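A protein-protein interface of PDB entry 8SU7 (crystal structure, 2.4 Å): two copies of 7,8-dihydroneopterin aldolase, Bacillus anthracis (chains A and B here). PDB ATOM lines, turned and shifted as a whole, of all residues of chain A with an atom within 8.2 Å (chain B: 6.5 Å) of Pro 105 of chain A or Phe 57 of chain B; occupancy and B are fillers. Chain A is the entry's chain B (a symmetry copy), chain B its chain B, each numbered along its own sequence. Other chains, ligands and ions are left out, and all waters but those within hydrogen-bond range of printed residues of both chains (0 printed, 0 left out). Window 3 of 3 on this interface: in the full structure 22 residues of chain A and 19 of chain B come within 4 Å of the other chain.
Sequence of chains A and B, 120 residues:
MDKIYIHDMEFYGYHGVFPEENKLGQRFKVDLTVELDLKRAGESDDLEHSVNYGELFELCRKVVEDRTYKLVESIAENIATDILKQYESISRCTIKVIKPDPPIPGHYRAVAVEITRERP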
ATOM      1  N   PRO A 102      -0.446  14.264  10.569  1.00  0.00           N
ATOM      2  CA  PRO A 102      -0.633  15.703  10.493  1.00  0.00           C
ATOM      3  C   PRO A 102       0.267  16.436  11.489  1.00  0.00           C
ATOM      4  O   PRO A 102       0.809  15.800  12.364  1.00  0.00           O
ATOM      5  CB  PRO A 102      -2.105  15.887  10.867  1.00  0.00           C
ATOM      6  CG  PRO A 102      -2.362  14.799  11.856  1.00  0.00           C
ATOM      7  CD  PRO A 102      -1.537  13.645  11.338  1.00  0.00           C
ATOM      8  N   PRO A 103       0.456  17.762  11.350  1.00  0.00           N
ATOM      9  CA  PRO A 103       1.242  18.527  12.314  1.00  0.00           C
ATOM     10  C   PRO A 103       0.365  18.886  13.528  1.00  0.00           C
ATOM     11  O   PRO A 103       0.132  20.058  13.724  1.00  0.00           O
ATOM     12  CB  PRO A 103       1.695  19.690  11.427  1.00  0.00           C
ATOM     13  CG  PRO A 103       0.509  19.959  10.538  1.00  0.00           C
ATOM     14  CD  PRO A 103      -0.076  18.590  10.272  1.00  0.00           C
ATOM     15  N   ILE A 104      -0.119  17.895  14.286  1.00  0.00           N
ATOM     16  CA  ILE A 104      -0.986  18.092  15.487  1.00  0.00           C
ATOM     17  C   ILE A 104      -0.231  17.589  16.729  1.00  0.00           C
ATOM     18  O   ILE A 104      -0.411  16.464  17.105  1.00  0.00           O
ATOM     19  CB  ILE A 104      -2.339  17.382  15.309  1.00  0.00           C
ATOM     20  CG1 ILE A 104      -3.101  17.872  14.076  1.00  0.00           C
ATOM     21  CG2 ILE A 104      -3.180  17.507  16.568  1.00  0.00           C
ATOM     22  CD1 ILE A 104      -4.241  16.967  13.676  1.00  0.00           C
ATOM     23  N   PRO A 105       0.588  18.383  17.435  1.00  0.00           N
ATOM     24  CA  PRO A 105       1.294  17.863  18.619  1.00  0.00           C
ATOM     25  C   PRO A 105       0.337  17.080  19.507  1.00  0.00           C
ATOM     26  O   PRO A 105      -0.620  17.631  20.057  1.00  0.00           O
ATOM     27  CB  PRO A 105       1.812  19.128  19.313  1.00  0.00           C
ATOM     28  CG  PRO A 105       1.868  20.173  18.230  1.00  0.00           C
ATOM     29  CD  PRO A 105       0.746  19.843  17.280  1.00  0.00           C
ATOM     30  N   GLY A 106       0.595  15.787  19.638  1.00  0.00           N
ATOM     31  CA  GLY A 106      -0.278  14.929  20.417  1.00  0.00           C
ATOM     32  C   GLY A 106      -0.053  13.473  20.049  1.00  0.00           C
ATOM     33  O   GLY A 106       0.964  13.120  19.458  1.00  0.00           O
ATOM     34  N   HIS A 107      -1.033  12.647  20.409  1.00  0.00           N
ATOM     35  CA  HIS A 107      -0.955  11.210  20.190  1.00  0.00           C
ATOM     36  C   HIS A 107      -2.299  10.713  19.687  1.00  0.00           C
ATOM     37  O   HIS A 107      -3.332  10.952  20.319  1.00  0.00           O
ATOM     38  CB  HIS A 107      -0.574  10.497  21.484  1.00  0.00           C
ATOM     39  CG  HIS A 107       0.755  10.914  22.033  1.00  0.00           C
ATOM     40  ND1 HIS A 107       1.940  10.341  21.624  1.00  0.00           N
ATOM     41  CD2 HIS A 107       1.085  11.843  22.960  1.00  0.00           C
ATOM     42  CE1 HIS A 107       2.944  10.899  22.278  1.00  0.00           C
ATOM     43  NE2 HIS A 107       2.453  11.815  23.092  1.00  0.00           N
ATOM     44  N   TYR A 108      -2.274  10.024  18.553  1.00  0.00           N
ATOM     45  CA  TYR A 108      -3.487   9.593  17.875  1.00  0.00           C
ATOM     46  C   TYR A 108      -3.071   8.643  16.764  1.00  0.00           C
ATOM     47  O   TYR A 108      -1.885   8.497  16.460  1.00  0.00           O
ATOM     48  CB  TYR A 108      -4.222  10.798  17.294  1.00  0.00           C
ATOM     49  CG  TYR A 108      -3.285  11.771  16.618  1.00  0.00           C
ATOM     50  CD1 TYR A 108      -2.750  11.493  15.368  1.00  0.00           C
ATOM     51  CD2 TYR A 108      -2.921  12.960  17.237  1.00  0.00           C
ATOM     52  CE1 TYR A 108      -1.890  12.371  14.749  1.00  0.00           C
ATOM     53  CE2 TYR A 108      -2.059  13.847  16.620  1.00  0.00           C
ATOM     54  CZ  TYR A 108      -1.548  13.546  15.378  1.00  0.00           C
ATOM     55  OH  TYR A 108      -0.690  14.424  14.764  1.00  0.00           O
ATOM     56  N   ARG A 109      -4.063   7.996  16.160  1.00  0.00           N
ATOM     57  CA  ARG A 109      -3.794   7.179  14.986  1.00  0.00           C
ATOM     58  C   ARG A 109      -3.877   8.010  13.710  1.00  0.00           C
ATOM     59  O   ARG A 109      -3.002   7.913  12.846  1.00  0.00           O
ATOM     60  CB  ARG A 109      -4.766   5.998  14.912  1.00  0.00           C
ATOM     61  CG  ARG A 109      -4.450   5.022  13.777  1.00  0.00           C
ATOM     62  CD  ARG A 109      -3.463   3.948  14.214  1.00  0.00           C
ATOM     63  NE  ARG A 109      -4.118   2.847  14.910  1.00  0.00           N
ATOM     64  CZ  ARG A 109      -3.865   2.490  16.162  1.00  0.00           C
ATOM     65  NH1 ARG A 109      -2.964   3.124  16.897  1.00  0.00           N
ATOM     66  NH2 ARG A 109      -4.535   1.470  16.691  1.00  0.00           N
ATOM     67  N   ALA A 110      -4.919   8.828  13.577  1.00  0.00           N
ATOM     68  CA  ALA A 110      -5.096   9.615  12.364  1.00  0.00           C
ATOM     69  C   ALA A 110      -6.248  10.588  12.557  1.00  0.00           C
ATOM     70  O   ALA A 110      -7.047  10.459  13.489  1.00  0.00           O
ATOM     71  CB  ALA A 110      -5.381   8.712  11.158  1.00  0.00           C
ATOM     72  N   VAL A 111      -6.298  11.585  11.677  1.00  0.00           N
ATOM     73  CA  VAL A 111      -7.476  12.415  11.469  1.00  0.00           C
ATOM     74  C   VAL A 111      -7.965  12.124  10.059  1.00  0.00           C
ATOM     75  O   VAL A 111      -7.168  11.814   9.166  1.00  0.00           O
ATOM     76  CB  VAL A 111      -7.192  13.920  11.665  1.00  0.00           C
ATOM     77  CG1 VAL A 111      -6.633  14.166  13.062  1.00  0.00           C
ATOM     78  CG2 VAL A 111      -6.249  14.428  10.597  1.00  0.00           C
ATOM     79  N   ILE B   6     -11.332  11.715  14.296  1.00  0.00           N
ATOM     80  CA  ILE B   6     -10.014  11.709  14.926  1.00  0.00           C
ATOM     81  C   ILE B   6      -9.872  10.341  15.576  1.00  0.00           C
ATOM     82  O   ILE B   6     -10.517  10.066  16.594  1.00  0.00           O
ATOM     83  CB  ILE B   6      -9.837  12.827  15.961  1.00  0.00           C
ATOM     84  CG1 ILE B   6     -10.031  14.191  15.296  1.00  0.00           C
ATOM     85  CG2 ILE B   6      -8.453  12.712  16.589  1.00  0.00           C
ATOM     86  CD1 ILE B   6      -9.355  15.356  16.012  1.00  0.00           C
ATOM     87  N   MET B   9      -7.096   8.742  19.732  1.00  0.00           N
ATOM     88  CA  MET B   9      -6.278   9.648  20.524  1.00  0.00           C
ATOM     89  C   MET B   9      -5.933   8.976  21.846  1.00  0.00           C
ATOM     90  O   MET B   9      -6.818   8.458  22.530  1.00  0.00           O
ATOM     91  CB  MET B   9      -7.041  10.940  20.800  1.00  0.00           C
ATOM     92  CG  MET B   9      -7.945  11.398  19.674  1.00  0.00           C
ATOM     93  SD  MET B   9      -8.720  12.986  20.022  1.00  0.00           S
ATOM     94  CE  MET B   9     -10.429  12.498  19.868  1.00  0.00           C
ATOM     95  N   GLU B  10      -4.652   8.976  22.207  1.00  0.00           N
ATOM     96  CA  GLU B  10      -4.189   8.358  23.443  1.00  0.00           C
ATOM     97  C   GLU B  10      -3.795   9.443  24.436  1.00  0.00           C
ATOM     98  O   GLU B  10      -2.993  10.327  24.115  1.00  0.00           O
ATOM     99  CB  GLU B  10      -2.998   7.430  23.194  1.00  0.00           C
ATOM    100  CG  GLU B  10      -2.326   6.956  24.477  1.00  0.00           C
ATOM    101  CD  GLU B  10      -1.599   5.633  24.322  1.00  0.00           C
ATOM    102  OE1 GLU B  10      -2.193   4.673  23.789  1.00  0.00           O
ATOM    103  OE2 GLU B  10      -0.431   5.552  24.745  1.00  0.00           O
ATOM    104  N   PHE B  11      -4.366   9.373  25.634  1.00  0.00           N
ATOM    105  CA  PHE B  11      -4.033  10.278  26.720  1.00  0.00           C
ATOM    106  C   PHE B  11      -3.681   9.458  27.953  1.00  0.00           C
ATOM    107  O   PHE B  11      -3.992   8.268  28.038  1.00  0.00           O
ATOM    108  CB  PHE B  11      -5.212  11.196  27.074  1.00  0.00           C
ATOM    109  CG  PHE B  11      -5.841  11.865  25.891  1.00  0.00           C
ATOM    110  CD1 PHE B  11      -5.203  12.914  25.252  1.00  0.00           C
ATOM    111  CD2 PHE B  11      -7.078  11.454  25.423  1.00  0.00           C
ATOM    112  CE1 PHE B  11      -5.779  13.534  24.160  1.00  0.00           C
ATOM    113  CE2 PHE B  11      -7.661  12.071  24.332  1.00  0.00           C
ATOM    114  CZ  PHE B  11      -7.010  13.114  23.701  1.00  0.00           C
ATOM    115  N   LEU B  32     -13.353  10.183  18.041  1.00  0.00           N
ATOM    116  CA  LEU B  32     -14.233  11.327  17.852  1.00  0.00           C
ATOM    117  C   LEU B  32     -14.811  11.298  16.446  1.00  0.00           C
ATOM    118  O   LEU B  32     -14.088  11.081  15.467  1.00  0.00           O
ATOM    119  CB  LEU B  32     -13.449  12.626  18.085  1.00  0.00           C
ATOM    120  CG  LEU B  32     -14.187  13.956  18.186  1.00  0.00           C
ATOM    121  CD1 LEU B  32     -13.232  15.062  18.657  1.00  0.00           C
ATOM    122  CD2 LEU B  32     -14.719  14.288  16.884  1.00  0.00           C
ATOM    123  N   ASN B  52     -11.281  23.085  12.193  1.00  0.00           N
ATOM    124  CA  ASN B  52      -9.897  22.699  12.453  1.00  0.00           C
ATOM    125  C   ASN B  52      -9.882  21.536  13.438  1.00  0.00           C
ATOM    126  O   ASN B  52     -10.242  21.698  14.608  1.00  0.00           O
ATOM    127  CB  ASN B  52      -9.134  23.891  13.024  1.00  0.00           C
ATOM    128  CG  ASN B  52      -7.667  23.589  13.256  1.00  0.00           C
ATOM    129  OD1 ASN B  52      -7.155  22.560  12.814  1.00  0.00           O
ATOM    130  ND2 ASN B  52      -6.979  24.488  13.951  1.00  0.00           N
ATOM    131  N   TYR B  53      -9.465  20.357  12.970  1.00  0.00           N
ATOM    132  CA  TYR B  53      -9.413  19.194  13.847  1.00  0.00           C
ATOM    133  C   TYR B  53      -8.279  19.281  14.856  1.00  0.00           C
ATOM    134  O   TYR B  53      -8.292  18.550  15.853  1.00  0.00           O
ATOM    135  CB  TYR B  53      -9.325  17.909  13.022  1.00  0.00           C
ATOM    136  CG  TYR B  53      -8.267  17.924  11.952  1.00  0.00           C
ATOM    137  CD1 TYR B  53      -6.954  17.920  12.281  1.00  0.00           C
ATOM    138  CD2 TYR B  53      -8.586  17.946  10.614  1.00  0.00           C
ATOM    139  CE1 TYR B  53      -5.958  17.940  11.311  1.00  0.00           C
ATOM    140  CE2 TYR B  53      -7.593  17.955   9.641  1.00  0.00           C
ATOM    141  CZ  TYR B  53      -6.277  17.948  10.007  1.00  0.00           C
ATOM    142  OH  TYR B  53      -5.272  17.952   9.071  1.00  0.00           O
ATOM    143  N   GLY B  54      -7.303  20.162  14.628  1.00  0.00           N
ATOM    144  CA  GLY B  54      -6.272  20.371  15.629  1.00  0.00           C
ATOM    145  C   GLY B  54      -6.836  20.962  16.907  1.00  0.00           C
ATOM    146  O   GLY B  54      -6.366  20.659  18.008  1.00  0.00           O
ATOM    147  N   GLU B  55      -7.844  21.825  16.776  1.00  0.00           N
ATOM    148  CA  GLU B  55      -8.561  22.297  17.954  1.00  0.00           C
ATOM    149  C   GLU B  55      -9.419  21.184  18.539  1.00  0.00           C
ATOM    150  O   GLU B  55      -9.494  21.025  19.763  1.00  0.00           O
ATOM    151  CB  GLU B  55      -9.446  23.489  17.592  1.00  0.00           C
ATOM    152  CG  GLU B  55      -8.696  24.746  17.186  1.00  0.00           C
ATOM    153  CD  GLU B  55      -9.563  25.706  16.387  1.00  0.00           C
ATOM    154  OE1 GLU B  55     -10.720  25.352  16.075  1.00  0.00           O
ATOM    155  OE2 GLU B  55      -9.088  26.817  16.072  1.00  0.00           O
ATOM    156  N   LEU B  56     -10.081  20.407  17.675  1.00  0.00           N
ATOM    157  CA  LEU B  56     -10.876  19.277  18.143  1.00  0.00           C
ATOM    158  C   LEU B  56     -10.040  18.347  19.011  1.00  0.00           C
ATOM    159  O   LEU B  56     -10.535  17.787  19.995  1.00  0.00           O
ATOM    160  CB  LEU B  56     -11.442  18.513  16.946  1.00  0.00           C
ATOM    161  CG  LEU B  56     -12.591  19.176  16.186  1.00  0.00           C
ATOM    162  CD1 LEU B  56     -12.705  18.618  14.769  1.00  0.00           C
ATOM    163  CD2 LEU B  56     -13.902  18.985  16.925  1.00  0.00           C
ATOM    164  N   PHE B  57      -8.763  18.177  18.665  1.00  0.00           N
ATOM    165  CA  PHE B  57      -7.882  17.356  19.486  1.00  0.00           C
ATOM    166  C   PHE B  57      -7.636  18.007  20.841  1.00  0.00           C
ATOM    167  O   PHE B  57      -7.716  17.347  21.883  1.00  0.00           O
ATOM    168  CB  PHE B  57      -6.554  17.126  18.762  1.00  0.00           C
ATOM    169  CG  PHE B  57      -5.523  16.431  19.602  1.00  0.00           C
ATOM    170  CD1 PHE B  57      -5.606  15.068  19.835  1.00  0.00           C
ATOM    171  CD2 PHE B  57      -4.469  17.138  20.157  1.00  0.00           C
ATOM    172  CE1 PHE B  57      -4.664  14.424  20.607  1.00  0.00           C
ATOM    173  CE2 PHE B  57      -3.524  16.498  20.931  1.00  0.00           C
ATOM    174  CZ  PHE B  57      -3.630  15.140  21.163  1.00  0.00           C
ATOM    175  N   GLU B  58      -7.329  19.308  20.845  1.00  0.00           N
ATOM    176  CA  GLU B  58      -7.028  19.989  22.099  1.00  0.00           C
ATOM    177  C   GLU B  58      -8.225  19.985  23.040  1.00  0.00           C
ATOM    178  O   GLU B  58      -8.052  19.936  24.262  1.00  0.00           O
ATOM    179  CB  GLU B  58      -6.579  21.423  21.822  1.00  0.00           C
ATOM    180  CG  GLU B  58      -6.271  22.231  23.073  1.00  0.00           C
ATOM    181  CD  GLU B  58      -5.172  21.615  23.916  1.00  0.00           C
ATOM    182  OE1 GLU B  58      -4.299  20.922  23.350  1.00  0.00           O
ATOM    183  OE2 GLU B  58      -5.186  21.817  25.147  1.00  0.00           O
ATOM    184  N   LEU B  59      -9.441  20.047  22.496  1.00  0.00           N
ATOM    185  CA  LEU B  59     -10.625  19.908  23.333  1.00  0.00           C
ATOM    186  C   LEU B  59     -10.611  18.578  24.077  1.00  0.00           C
ATOM    187  O   LEU B  59     -10.801  18.529  25.290  1.00  0.00           O
ATOM    188  CB  LEU B  59     -11.884  20.006  22.474  1.00  0.00           C
ATOM    189  CG  LEU B  59     -13.092  20.723  23.075  1.00  0.00           C
ATOM    190  CD1 LEU B  59     -12.808  22.207  23.216  1.00  0.00           C
ATOM    191  CD2 LEU B  59     -14.333  20.491  22.217  1.00  0.00           C
ATOM    192  N   CYS B  60     -10.407  17.475  23.372  1.00  0.00           N
ATOM    193  CA  CYS B  60     -10.396  16.193  24.072  1.00  0.00           C
ATOM    194  C   CYS B  60      -9.208  16.081  25.023  1.00  0.00           C
ATOM    195  O   CYS B  60      -9.305  15.451  26.085  1.00  0.00           O
ATOM    196  CB  CYS B  60     -10.371  15.068  23.050  1.00  0.00           C
ATOM    197  SG  CYS B  60     -11.763  15.112  21.921  1.00  0.00           S
ATOM    198  N   ARG B  61      -8.075  16.679  24.658  1.00  0.00           N
ATOM    199  CA  ARG B  61      -6.902  16.630  25.524  1.00  0.00           C
ATOM    200  C   ARG B  61      -7.202  17.249  26.884  1.00  0.00           C
ATOM    201  O   ARG B  61      -6.839  16.695  27.927  1.00  0.00           O
ATOM    202  CB  ARG B  61      -5.742  17.362  24.851  1.00  0.00           C
ATOM    203  CG  ARG B  61      -4.363  16.902  25.285  1.00  0.00           C
ATOM    204  CD  ARG B  61      -3.349  18.040  25.193  1.00  0.00           C
ATOM    205  NE  ARG B  61      -3.783  19.210  25.948  1.00  0.00           N
ATOM    206  CZ  ARG B  61      -3.834  19.267  27.271  1.00  0.00           C
ATOM    207  NH1 ARG B  61      -3.445  18.250  28.021  1.00  0.00           N
ATOM    208  NH2 ARG B  61      -4.291  20.371  27.855  1.00  0.00           N
ATOM    209  N   LYS B  62      -7.874  18.397  26.891  1.00  0.00           N
ATOM    210  CA  LYS B  62      -8.150  19.069  28.154  1.00  0.00           C
ATOM    211  C   LYS B  62      -9.115  18.268  29.014  1.00  0.00           C
ATOM    212  O   LYS B  62      -8.905  18.129  30.223  1.00  0.00           O
ATOM    213  CB  LYS B  62      -8.716  20.458  27.884  1.00  0.00           C
ATOM    214  CG  LYS B  62     -10.142  20.468  27.325  1.00  0.00           C
ATOM    215  CD  LYS B  62     -10.413  21.716  26.494  1.00  0.00           C
ATOM    216  CE  LYS B  62     -10.076  22.987  27.266  1.00  0.00           C
ATOM    217  NZ  LYS B  62     -10.996  23.188  28.428  1.00  0.00           N
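O of His 107 of chain A is in hydrogen-bond range of N of Glu 10 of chain B (3.0 Å).
O of Pro 102 of chain A is in hydrogen-bond range of OH of Tyr 108 of chain A.
N of Ile 6 of chain B is in hydrogen-bond range of O of Leu 32 of chain B (3.1 Å).
O of Ile 104 of chain A lies within hydrogen-bond range of OH of Tyr 108 of chain A (3.1 Å).
Ile 104 of chain A touches Tyr 53 of chain B (CD1 to CE1, 3.1 Å).
Ile 104 of chain A touches Phe 57 of chain B (CG2 to CD2, 3.8 Å).
Phe 57 of chain B touches Pro 105 of chain A.
Gly 106 of chain A touches Phe 57 of chain B.
His 107 of chain A touches Met 9 of chain B.
His 107 of chain A touches Phe 57 of chain B.
CA of Tyr 108 of chain A touches CA of Met 9 of chain B (3.8 Å).
Ala 110 of chain A touches Ile 6 of chain B (O to C, 3.5 Å).
Val 111 of chain A touches Tyr 53 of chain B.
Of chain B, only Phe 57 (3.2 Å) comes within 4 Å of Pro 105 of chain A.
Of the printed residues of chain A, Phe 57 of chain B touches Ile 104, Pro 105, Gly 106 and His 107.
Of the printed residues of chain A, Met 9 of chain B touches His 107 and Tyr 108.
Of the printed residues of chain A, Tyr 53 of chain B touches Ile 104 (3.1 Å) and Val 111 (3.6 Å).
Pro 103 of chain A touches none of the printed residues of chain B.
The nearest residue of chain B that does not touch Pro 105 of chain A is Arg 61 of chain B (5.8 Å).
The nearest printed residue of chain B that does not touch Val 111 of chain A is Ile 6 of chain B (4.1 Å).
Of the 16 printed residues of chain B, 5 touch a printed residue of chain A.
Hydrophobic or aromatic side chains of chain B within 4 Å of the printed part of chain A: Met 9, Tyr 53 and Phe 57.
Hydrophobic or aromatic side chains of chain A that line the printed part of chain B: Ile 104, His 107, Tyr 108 and Val 111.
Among the printed residues, 10 pairs touch across the chains.
No position is printed for both chains.
Of the 10 pairs that touch across the chains among the printed residues, none has its exchanged pair printed and touching as well.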
